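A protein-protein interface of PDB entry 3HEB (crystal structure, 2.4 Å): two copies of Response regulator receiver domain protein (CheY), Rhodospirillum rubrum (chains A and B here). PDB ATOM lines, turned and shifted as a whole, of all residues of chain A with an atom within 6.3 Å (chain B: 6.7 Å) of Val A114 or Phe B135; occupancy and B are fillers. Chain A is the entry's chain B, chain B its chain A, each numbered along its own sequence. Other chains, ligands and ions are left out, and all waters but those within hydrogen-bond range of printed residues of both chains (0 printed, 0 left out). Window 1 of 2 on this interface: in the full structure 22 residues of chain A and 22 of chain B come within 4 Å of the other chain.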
ATOM      1  N   VAL A  92      -1.301   3.778 -27.346  1.00  0.00           N
ATOM      2  CA  VAL A  92      -2.663   4.263 -27.228  1.00  0.00           C
ATOM      3  C   VAL A  92      -2.659   5.766 -27.035  1.00  0.00           C
ATOM      4  O   VAL A  92      -2.020   6.281 -26.111  1.00  0.00           O
ATOM      5  CB  VAL A  92      -3.397   3.624 -26.021  1.00  0.00           C
ATOM      6  CG1 VAL A  92      -4.791   4.240 -25.871  1.00  0.00           C
ATOM      7  CG2 VAL A  92      -3.509   2.117 -26.215  1.00  0.00           C
ATOM      8  N   VAL A  93      -3.370   6.462 -27.915  1.00  0.00           N
ATOM      9  CA  VAL A  93      -3.486   7.907 -27.846  1.00  0.00           C
ATOM     10  C   VAL A  93      -4.916   8.254 -27.487  1.00  0.00           C
ATOM     11  O   VAL A  93      -5.839   7.961 -28.245  1.00  0.00           O
ATOM     12  CB  VAL A  93      -3.176   8.593 -29.193  1.00  0.00           C
ATOM     13  CG1 VAL A  93      -3.457  10.096 -29.078  1.00  0.00           C
ATOM     14  CG2 VAL A  93      -1.720   8.377 -29.581  1.00  0.00           C
ATOM     15  N   ILE A  94      -5.101   8.872 -26.330  1.00  0.00           N
ATOM     16  CA  ILE A  94      -6.425   9.280 -25.898  1.00  0.00           C
ATOM     17  C   ILE A  94      -6.731  10.576 -26.631  1.00  0.00           C
ATOM     18  O   ILE A  94      -5.929  11.507 -26.625  1.00  0.00           O
ATOM     19  CB  ILE A  94      -6.461   9.569 -24.393  1.00  0.00           C
ATOM     20  CG1 ILE A  94      -5.968   8.349 -23.596  1.00  0.00           C
ATOM     21  CG2 ILE A  94      -7.867   9.949 -23.990  1.00  0.00           C
ATOM     22  CD1 ILE A  94      -6.902   7.161 -23.612  1.00  0.00           C
ATOM     23  N   LEU A  95      -7.878  10.629 -27.294  1.00  0.00           N
ATOM     24  CA  LEU A  95      -8.259  11.834 -28.004  1.00  0.00           C
ATOM     25  C   LEU A  95      -9.691  12.063 -27.585  1.00  0.00           C
ATOM     26  O   LEU A  95     -10.623  11.538 -28.201  1.00  0.00           O
ATOM     27  CB  LEU A  95      -8.149  11.624 -29.518  1.00  0.00           C
ATOM     28  CG  LEU A  95      -8.554  12.787 -30.432  1.00  0.00           C
ATOM     29  CD1 LEU A  95      -7.867  14.081 -29.996  1.00  0.00           C
ATOM     30  CD2 LEU A  95      -8.201  12.433 -31.869  1.00  0.00           C
ATOM     31  N   TYR A 108      -2.764   8.192 -17.936  1.00  0.00           N
ATOM     32  CA  TYR A 108      -1.347   7.901 -18.059  1.00  0.00           C
ATOM     33  C   TYR A 108      -0.973   6.735 -17.149  1.00  0.00           C
ATOM     34  O   TYR A 108      -0.264   5.827 -17.568  1.00  0.00           O
ATOM     35  CB  TYR A 108      -0.505   9.149 -17.763  1.00  0.00           C
ATOM     36  CG  TYR A 108      -0.432  10.106 -18.944  1.00  0.00           C
ATOM     37  CD1 TYR A 108      -1.180  11.287 -18.977  1.00  0.00           C
ATOM     38  CD2 TYR A 108       0.373   9.805 -20.049  1.00  0.00           C
ATOM     39  CE1 TYR A 108      -1.120  12.147 -20.093  1.00  0.00           C
ATOM     40  CE2 TYR A 108       0.436  10.647 -21.160  1.00  0.00           C
ATOM     41  CZ  TYR A 108      -0.307  11.810 -21.177  1.00  0.00           C
ATOM     42  OH  TYR A 108      -0.219  12.621 -22.277  1.00  0.00           O
ATOM     43  N   GLY A 111      -1.567   3.474 -18.513  1.00  0.00           N
ATOM     44  CA  GLY A 111      -0.735   3.078 -19.638  1.00  0.00           C
ATOM     45  C   GLY A 111      -0.928   3.806 -20.954  1.00  0.00           C
ATOM     46  O   GLY A 111      -0.423   3.359 -21.981  1.00  0.00           O
ATOM     47  N   ALA A 112      -1.659   4.912 -20.946  1.00  0.00           N
ATOM     48  CA  ALA A 112      -1.854   5.654 -22.178  1.00  0.00           C
ATOM     49  C   ALA A 112      -0.497   6.227 -22.585  1.00  0.00           C
ATOM     50  O   ALA A 112       0.272   6.677 -21.732  1.00  0.00           O
ATOM     51  CB  ALA A 112      -2.855   6.773 -21.966  1.00  0.00           C
ATOM     52  N   ASN A 113      -0.202   6.203 -23.880  1.00  0.00           N
ATOM     53  CA  ASN A 113       1.060   6.729 -24.388  1.00  0.00           C
ATOM     54  C   ASN A 113       0.991   8.242 -24.509  1.00  0.00           C
ATOM     55  O   ASN A 113       1.957   8.945 -24.194  1.00  0.00           O
ATOM     56  CB  ASN A 113       1.375   6.147 -25.775  1.00  0.00           C
ATOM     57  CG  ASN A 113       1.715   4.673 -25.735  1.00  0.00           C
ATOM     58  OD1 ASN A 113       2.886   4.293 -25.809  1.00  0.00           O
ATOM     59  ND2 ASN A 113       0.685   3.828 -25.611  1.00  0.00           N
ATOM     60  N   VAL A 114      -0.151   8.727 -24.989  1.00  0.00           N
ATOM     61  CA  VAL A 114      -0.387  10.151 -25.197  1.00  0.00           C
ATOM     62  C   VAL A 114      -1.857  10.490 -24.925  1.00  0.00           C
ATOM     63  O   VAL A 114      -2.771   9.729 -25.264  1.00  0.00           O
ATOM     64  CB  VAL A 114      -0.049  10.571 -26.668  1.00  0.00           C
ATOM     65  CG1 VAL A 114      -0.517  12.000 -26.935  1.00  0.00           C
ATOM     66  CG2 VAL A 114       1.449  10.455 -26.929  1.00  0.00           C
ATOM     67  N   TYR A 115      -2.080  11.632 -24.294  1.00  0.00           N
ATOM     68  CA  TYR A 115      -3.433  12.074 -24.007  1.00  0.00           C
ATOM     69  C   TYR A 115      -3.592  13.427 -24.679  1.00  0.00           C
ATOM     70  O   TYR A 115      -2.755  14.318 -24.510  1.00  0.00           O
ATOM     71  CB  TYR A 115      -3.658  12.213 -22.500  1.00  0.00           C
ATOM     72  CG  TYR A 115      -5.080  12.589 -22.130  1.00  0.00           C
ATOM     73  CD1 TYR A 115      -5.891  11.714 -21.410  1.00  0.00           C
ATOM     74  CD2 TYR A 115      -5.608  13.829 -22.489  1.00  0.00           C
ATOM     75  CE1 TYR A 115      -7.186  12.066 -21.054  1.00  0.00           C
ATOM     76  CE2 TYR A 115      -6.898  14.188 -22.139  1.00  0.00           C
ATOM     77  CZ  TYR A 115      -7.680  13.307 -21.421  1.00  0.00           C
ATOM     78  OH  TYR A 115      -8.951  13.684 -21.049  1.00  0.00           O
ATOM     79  N   ILE A 116      -4.661  13.570 -25.448  1.00  0.00           N
ATOM     80  CA  ILE A 116      -4.935  14.820 -26.139  1.00  0.00           C
ATOM     81  C   ILE A 116      -6.377  15.267 -25.908  1.00  0.00           C
ATOM     82  O   ILE A 116      -7.318  14.495 -26.094  1.00  0.00           O
ATOM     83  CB  ILE A 116      -4.714  14.665 -27.663  1.00  0.00           C
ATOM     84  CG1 ILE A 116      -3.254  14.292 -27.942  1.00  0.00           C
ATOM     85  CG2 ILE A 116      -5.099  15.944 -28.378  1.00  0.00           C
ATOM     86  CD1 ILE A 116      -2.940  14.039 -29.406  1.00  0.00           C
ATOM     87  N   ALA A 128      -4.936  20.066 -34.940  1.00  0.00           N
ATOM     88  CA  ALA A 128      -4.367  19.151 -33.957  1.00  0.00           C
ATOM     89  C   ALA A 128      -4.274  17.729 -34.525  1.00  0.00           C
ATOM     90  O   ALA A 128      -3.254  17.057 -34.367  1.00  0.00           O
ATOM     91  CB  ALA A 128      -5.210  19.160 -32.678  1.00  0.00           C
ATOM     92  N   GLN A 131      -1.481  17.560 -36.951  1.00  0.00           N
ATOM     93  CA  GLN A 131      -0.178  17.437 -36.290  1.00  0.00           C
ATOM     94  C   GLN A 131       0.036  15.994 -35.856  1.00  0.00           C
ATOM     95  O   GLN A 131       1.130  15.453 -36.001  1.00  0.00           O
ATOM     96  CB  GLN A 131      -0.077  18.348 -35.059  1.00  0.00           C
ATOM     97  CG  GLN A 131      -0.112  19.824 -35.382  1.00  0.00           C
ATOM     98  CD  GLN A 131       0.745  20.183 -36.584  1.00  0.00           C
ATOM     99  OE1 GLN A 131       1.898  19.760 -36.689  1.00  0.00           O
ATOM    100  NE2 GLN A 131       0.185  20.975 -37.496  1.00  0.00           N
ATOM    101  N   LEU A 132      -1.018  15.381 -35.319  1.00  0.00           N
ATOM    102  CA  LEU A 132      -0.980  13.982 -34.884  1.00  0.00           C
ATOM    103  C   LEU A 132      -0.538  13.090 -36.047  1.00  0.00           C
ATOM    104  O   LEU A 132       0.286  12.187 -35.876  1.00  0.00           O
ATOM    105  CB  LEU A 132      -2.368  13.531 -34.442  1.00  0.00           C
ATOM    106  CG  LEU A 132      -2.545  12.323 -33.523  1.00  0.00           C
ATOM    107  CD1 LEU A 132      -3.913  11.725 -33.812  1.00  0.00           C
ATOM    108  CD2 LEU A 132      -1.455  11.294 -33.724  1.00  0.00           C
ATOM    109  N   GLY A 133      -1.106  13.347 -37.225  1.00  0.00           N
ATOM    110  CA  GLY A 133      -0.767  12.553 -38.394  1.00  0.00           C
ATOM    111  C   GLY A 133       0.699  12.693 -38.764  1.00  0.00           C
ATOM    112  O   GLY A 133       1.354  11.725 -39.148  1.00  0.00           O
ATOM    113  N   PHE A 135       3.106  13.630 -36.653  1.00  0.00           N
ATOM    114  CA  PHE A 135       3.895  13.012 -35.603  1.00  0.00           C
ATOM    115  C   PHE A 135       3.908  11.493 -35.786  1.00  0.00           C
ATOM    116  O   PHE A 135       4.930  10.846 -35.587  1.00  0.00           O
ATOM    117  CB  PHE A 135       3.332  13.345 -34.231  1.00  0.00           C
ATOM    118  CG  PHE A 135       4.246  12.969 -33.118  1.00  0.00           C
ATOM    119  CD1 PHE A 135       5.498  13.567 -33.006  1.00  0.00           C
ATOM    120  CD2 PHE A 135       3.875  12.010 -32.189  1.00  0.00           C
ATOM    121  CE1 PHE A 135       6.364  13.215 -31.980  1.00  0.00           C
ATOM    122  CE2 PHE A 135       4.738  11.653 -31.155  1.00  0.00           C
ATOM    123  CZ  PHE A 135       5.982  12.254 -31.054  1.00  0.00           C
ATOM    124  N   ALA B  27       9.425  25.428 -33.684  1.00  0.00           N
ATOM    125  CA  ALA B  27       8.027  25.020 -33.646  1.00  0.00           C
ATOM    126  C   ALA B  27       7.162  25.948 -32.793  1.00  0.00           C
ATOM    127  O   ALA B  27       5.952  25.744 -32.671  1.00  0.00           O
ATOM    128  CB  ALA B  27       7.926  23.591 -33.132  1.00  0.00           C
ATOM    129  N   PRO B  91       5.823  11.676 -19.374  1.00  0.00           N
ATOM    130  CA  PRO B  91       5.969  11.052 -20.688  1.00  0.00           C
ATOM    131  C   PRO B  91       7.438  11.015 -21.096  1.00  0.00           C
ATOM    132  O   PRO B  91       8.181  11.974 -20.891  1.00  0.00           O
ATOM    133  CB  PRO B  91       5.121  11.944 -21.602  1.00  0.00           C
ATOM    134  CG  PRO B  91       5.103  13.248 -20.896  1.00  0.00           C
ATOM    135  CD  PRO B  91       4.945  12.853 -19.454  1.00  0.00           C
ATOM    136  N   ASN B 113       6.748   6.326 -23.683  1.00  0.00           N
ATOM    137  CA  ASN B 113       5.489   6.786 -24.266  1.00  0.00           C
ATOM    138  C   ASN B 113       5.565   6.803 -25.783  1.00  0.00           C
ATOM    139  O   ASN B 113       4.592   6.498 -26.466  1.00  0.00           O
ATOM    140  CB  ASN B 113       5.157   8.199 -23.780  1.00  0.00           C
ATOM    141  CG  ASN B 113       4.837   8.246 -22.294  1.00  0.00           C
ATOM    142  OD1 ASN B 113       3.664   8.277 -21.885  1.00  0.00           O
ATOM    143  ND2 ASN B 113       5.883   8.236 -21.473  1.00  0.00           N
ATOM    144  N   VAL B 114       6.732   7.180 -26.291  1.00  0.00           N
ATOM    145  CA  VAL B 114       6.978   7.290 -27.721  1.00  0.00           C
ATOM    146  C   VAL B 114       8.444   6.991 -28.020  1.00  0.00           C
ATOM    147  O   VAL B 114       9.330   7.246 -27.200  1.00  0.00           O
ATOM    148  CB  VAL B 114       6.663   8.716 -28.224  1.00  0.00           C
ATOM    149  CG1 VAL B 114       6.967   8.840 -29.723  1.00  0.00           C
ATOM    150  CG2 VAL B 114       5.207   9.058 -27.933  1.00  0.00           C
ATOM    151  N   ARG B 130      10.808  19.448 -35.213  1.00  0.00           N
ATOM    152  CA  ARG B 130       9.853  20.532 -35.344  1.00  0.00           C
ATOM    153  C   ARG B 130       8.478  19.881 -35.173  1.00  0.00           C
ATOM    154  O   ARG B 130       7.608  20.384 -34.454  1.00  0.00           O
ATOM    155  CB  ARG B 130      10.011  21.132 -36.735  1.00  0.00           C
ATOM    156  CG  ARG B 130       9.315  22.435 -37.013  1.00  0.00           C
ATOM    157  CD  ARG B 130       9.815  22.921 -38.383  1.00  0.00           C
ATOM    158  NE  ARG B 130      11.274  23.018 -38.385  1.00  0.00           N
ATOM    159  CZ  ARG B 130      12.073  22.563 -39.349  1.00  0.00           C
ATOM    160  NH1 ARG B 130      11.575  21.965 -40.425  1.00  0.00           N
ATOM    161  NH2 ARG B 130      13.382  22.700 -39.228  1.00  0.00           N
ATOM    162  N   GLN B 131       8.304  18.734 -35.820  1.00  0.00           N
ATOM    163  CA  GLN B 131       7.054  17.993 -35.746  1.00  0.00           C
ATOM    164  C   GLN B 131       6.789  17.544 -34.310  1.00  0.00           C
ATOM    165  O   GLN B 131       5.645  17.527 -33.864  1.00  0.00           O
ATOM    166  CB  GLN B 131       7.111  16.788 -36.677  1.00  0.00           C
ATOM    167  CG  GLN B 131       5.854  16.586 -37.477  1.00  0.00           C
ATOM    168  CD  GLN B 131       5.346  17.888 -38.080  1.00  0.00           C
ATOM    169  OE1 GLN B 131       4.376  18.473 -37.591  1.00  0.00           O
ATOM    170  NE2 GLN B 131       6.011  18.354 -39.139  1.00  0.00           N
ATOM    171  N   LEU B 132       7.857  17.188 -33.601  1.00  0.00           N
ATOM    172  CA  LEU B 132       7.786  16.758 -32.201  1.00  0.00           C
ATOM    173  C   LEU B 132       7.333  17.951 -31.324  1.00  0.00           C
ATOM    174  O   LEU B 132       6.512  17.802 -30.409  1.00  0.00           O
ATOM    175  CB  LEU B 132       9.178  16.289 -31.749  1.00  0.00           C
ATOM    176  CG  LEU B 132       9.416  15.463 -30.472  1.00  0.00           C
ATOM    177  CD1 LEU B 132      10.824  15.745 -29.966  1.00  0.00           C
ATOM    178  CD2 LEU B 132       8.426  15.811 -29.401  1.00  0.00           C
ATOM    179  N   GLY B 133       7.886  19.128 -31.615  1.00  0.00           N
ATOM    180  CA  GLY B 133       7.545  20.327 -30.869  1.00  0.00           C
ATOM    181  C   GLY B 133       6.095  20.726 -31.069  1.00  0.00           C
ATOM    182  O   GLY B 133       5.426  21.128 -30.123  1.00  0.00           O
ATOM    183  N   LEU B 134       5.604  20.614 -32.297  1.00  0.00           N
ATOM    184  CA  LEU B 134       4.221  20.954 -32.599  1.00  0.00           C
ATOM    185  C   LEU B 134       3.261  20.036 -31.854  1.00  0.00           C
ATOM    186  O   LEU B 134       2.271  20.494 -31.301  1.00  0.00           O
ATOM    187  CB  LEU B 134       3.964  20.854 -34.105  1.00  0.00           C
ATOM    188  CG  LEU B 134       4.614  21.977 -34.914  1.00  0.00           C
ATOM    189  CD1 LEU B 134       4.459  21.723 -36.404  1.00  0.00           C
ATOM    190  CD2 LEU B 134       3.968  23.307 -34.508  1.00  0.00           C
ATOM    191  N   PHE B 135       3.562  18.741 -31.852  1.00  0.00           N
ATOM    192  CA  PHE B 135       2.735  17.745 -31.177  1.00  0.00           C
ATOM    193  C   PHE B 135       2.734  17.987 -29.672  1.00  0.00           C
ATOM    194  O   PHE B 135       1.702  17.890 -29.017  1.00  0.00           O
ATOM    195  CB  PHE B 135       3.275  16.348 -31.462  1.00  0.00           C
ATOM    196  CG  PHE B 135       2.339  15.252 -31.074  1.00  0.00           C
ATOM    197  CD1 PHE B 135       1.084  15.148 -31.673  1.00  0.00           C
ATOM    198  CD2 PHE B 135       2.713  14.308 -30.126  1.00  0.00           C
ATOM    199  CE1 PHE B 135       0.214  14.111 -31.327  1.00  0.00           C
ATOM    200  CE2 PHE B 135       1.857  13.272 -29.774  1.00  0.00           C
ATOM    201  CZ  PHE B 135       0.604  13.170 -30.373  1.00  0.00           C
ATOM    202  N   PHE B 136       3.907  18.294 -29.137  1.00  0.00           N
ATOM    203  CA  PHE B 136       4.066  18.576 -27.723  1.00  0.00           C
ATOM    204  C   PHE B 136       3.065  19.651 -27.298  1.00  0.00           C
ATOM    205  O   PHE B 136       2.399  19.538 -26.272  1.00  0.00           O
ATOM    206  CB  PHE B 136       5.490  19.082 -27.464  1.00  0.00           C
ATOM    207  CG  PHE B 136       5.682  19.676 -26.097  1.00  0.00           C
ATOM    208  CD1 PHE B 136       5.891  18.856 -24.988  1.00  0.00           C
ATOM    209  CD2 PHE B 136       5.630  21.061 -25.910  1.00  0.00           C
ATOM    210  CE1 PHE B 136       6.043  19.400 -23.719  1.00  0.00           C
ATOM    211  CE2 PHE B 136       5.783  21.617 -24.639  1.00  0.00           C
ATOM    212  CZ  PHE B 136       5.989  20.781 -23.542  1.00  0.00           C
ATOM    213  N   SER B 137       2.959  20.698 -28.102  1.00  0.00           N
ATOM    214  CA  SER B 137       2.063  21.799 -27.781  1.00  0.00           C
ATOM    215  C   SER B 137       0.599  21.424 -27.942  1.00  0.00           C
ATOM    216  O   SER B 137      -0.285  22.192 -27.565  1.00  0.00           O
ATOM    217  CB  SER B 137       2.390  23.003 -28.662  1.00  0.00           C
ATOM    218  OG  SER B 137       2.065  22.724 -30.009  1.00  0.00           O
ATOM    219  N   VAL B 138       0.349  20.240 -28.490  1.00  0.00           N
ATOM    220  CA  VAL B 138      -1.013  19.759 -28.710  1.00  0.00           C
ATOM    221  C   VAL B 138      -1.460  18.735 -27.656  1.00  0.00           C
ATOM    222  O   VAL B 138      -2.656  18.596 -27.379  1.00  0.00           O
ATOM    223  CB  VAL B 138      -1.123  19.121 -30.121  1.00  0.00           C
ATOM    224  CG1 VAL B 138      -2.255  18.115 -30.169  1.00  0.00           C
ATOM    225  CG2 VAL B 138      -1.333  20.207 -31.168  1.00  0.00           C
ATOM    226  N   MET B 139      -0.494  18.031 -27.069  1.00  0.00           N
ATOM    227  CA  MET B 139      -0.760  16.998 -26.069  1.00  0.00           C
ATOM    228  C   MET B 139      -0.827  17.523 -24.642  1.00  0.00           C
ATOM    229  O   MET B 139      -0.395  18.639 -24.358  1.00  0.00           O
ATOM    230  CB  MET B 139       0.321  15.899 -26.141  1.00  0.00           C
ATOM    231  CG  MET B 139       1.723  16.324 -25.716  1.00  0.00           C
ATOM    232  SD  MET B 139       2.995  15.038 -25.962  1.00  0.00           S
ATOM    233  CE  MET B 139       2.972  14.269 -24.385  1.00  0.00           C
ATOM    234  N   GLN B 140      -1.384  16.707 -23.750  1.00  0.00           N
ATOM    235  CA  GLN B 140      -1.472  17.043 -22.330  1.00  0.00           C
ATOM    236  C   GLN B 140      -0.293  16.374 -21.613  1.00  0.00           C
ATOM    237  O   GLN B 140      -0.110  15.163 -21.728  1.00  0.00           O
ATOM    238  CB  GLN B 140      -2.764  16.495 -21.728  1.00  0.00           C
ATOM    239  CG  GLN B 140      -4.038  17.106 -22.253  1.00  0.00           C
ATOM    240  CD  GLN B 140      -4.417  18.370 -21.520  1.00  0.00           C
ATOM    241  OE1 GLN B 140      -5.466  18.957 -21.787  1.00  0.00           O
ATOM    242  NE2 GLN B 140      -3.573  18.798 -20.582  1.00  0.00           N
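O of Gln B140 lies within hydrogen-bond range of OH of Tyr A108, 2.6 Å away. The backbone carbonyl oxygen (O) of Asn B113 sits close to the side-chain amide oxygen (OD1) of Asn A113 (2.9 Å). OE1 of Gln B131 sits close to OE1 of Gln A131 (2.9 Å). N of Gln B140 lies within hydrogen-bond range of O of Tyr A115, 2.9 Å away.
Of chain B, only Phe B135 (3.8 Å) comes within 4 Å of Val A114. Of the printed residues of chain B, Ile A116 touches Phe B135 and Val B138. Of the printed residues of chain A, Asn B113 touches Ala A112 and Asn A113. Of the printed residues of chain A, Val B114 touches Phe A135. Of the printed residues of chain A, Leu B134 touches Gln A131 (3.2 Å). Phe B135 touches four residues of chain A. The nearest residue of chain A that does not touch Phe B135 is Gln A131 (4.3 Å). The nearest printed residue of chain A that does not touch Val B138 is Ala A128 (4.01 Å).
Asn A113 touches its own counterpart, Asn B113. Val A114 touches Phe B135, and with the chains exchanged Phe A135 touches Val B114. Gln B131 touches its own counterpart, Gln A131. Leu A132 touches Phe B135, and with the chains exchanged Phe A135 touches Leu B132. Of the 14 pairs that touch across the chains among the printed residues, 7 have their exchanged pair printed and touching as well.
The backbone carbonyl oxygen (O) of Ile A94 is in hydrogen-bond range of the backbone NH (N) of Ile A116, 2.7 Å away. N of Ile A94 lies within hydrogen-bond range of O of Val A114, at 2.7 Å. The backbone carbonyl oxygen (O) of Val A92 sits at hydrogen-bond distance from the backbone NH (N) of Val A114. The side-chain hydroxyl (OG) of Ser B137 is in hydrogen-bond range of the backbone carbonyl oxygen (O) of Leu B134, 2.6 Å away. The backbone NH (N) of Val A92 sits close to the side-chain amide nitrogen (ND2) of Asn A113 (2.6 Å). OH of Tyr A108 is in hydrogen-bond range of N of Tyr A115 (2.9 Å).
Among the printed residues, merely in contact across the chains: Gln A131 with Leu B134 (3.2 Å), Phe A135 with Phe B135 (3.3 Å), Tyr A115 with Met B139 (3.7 Å), Ile A116 with Phe B135 (3.7 Å), Ile A116 with Val B138 (3.7 Å), Ala A112 with Asn B113 (3.8 Å), Leu A132 with Phe B135 (3.8 Å), Phe A135 with Val B114 (3.8 Å), Val A114 with Phe B135 (3.8 Å) and Phe A135 with Leu B132 (3.8 Å).
Of the 15 printed residues of chain B, 9 touch a printed residue of chain A. Hydrophobic or aromatic side chains of chain B within 4 Å of the printed part of chain A: Val B114, Leu B134, Phe B135 and Met B139. Of the 16 printed residues of chain A, 9 touch a printed residue of chain B. Hydrophobic or aromatic side chains of chain A that line the printed part of chain B: Tyr A108, Val A114, Tyr A115, Ile A116, Leu A132 and Phe A135. Along chain A the printed residues that touch a printed residue of chain B span positions 108 to 135. Among the printed residues, no Asp or Glu carboxylate lies within 4 Å of a Lys or Arg side-chain nitrogen of the other chain.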
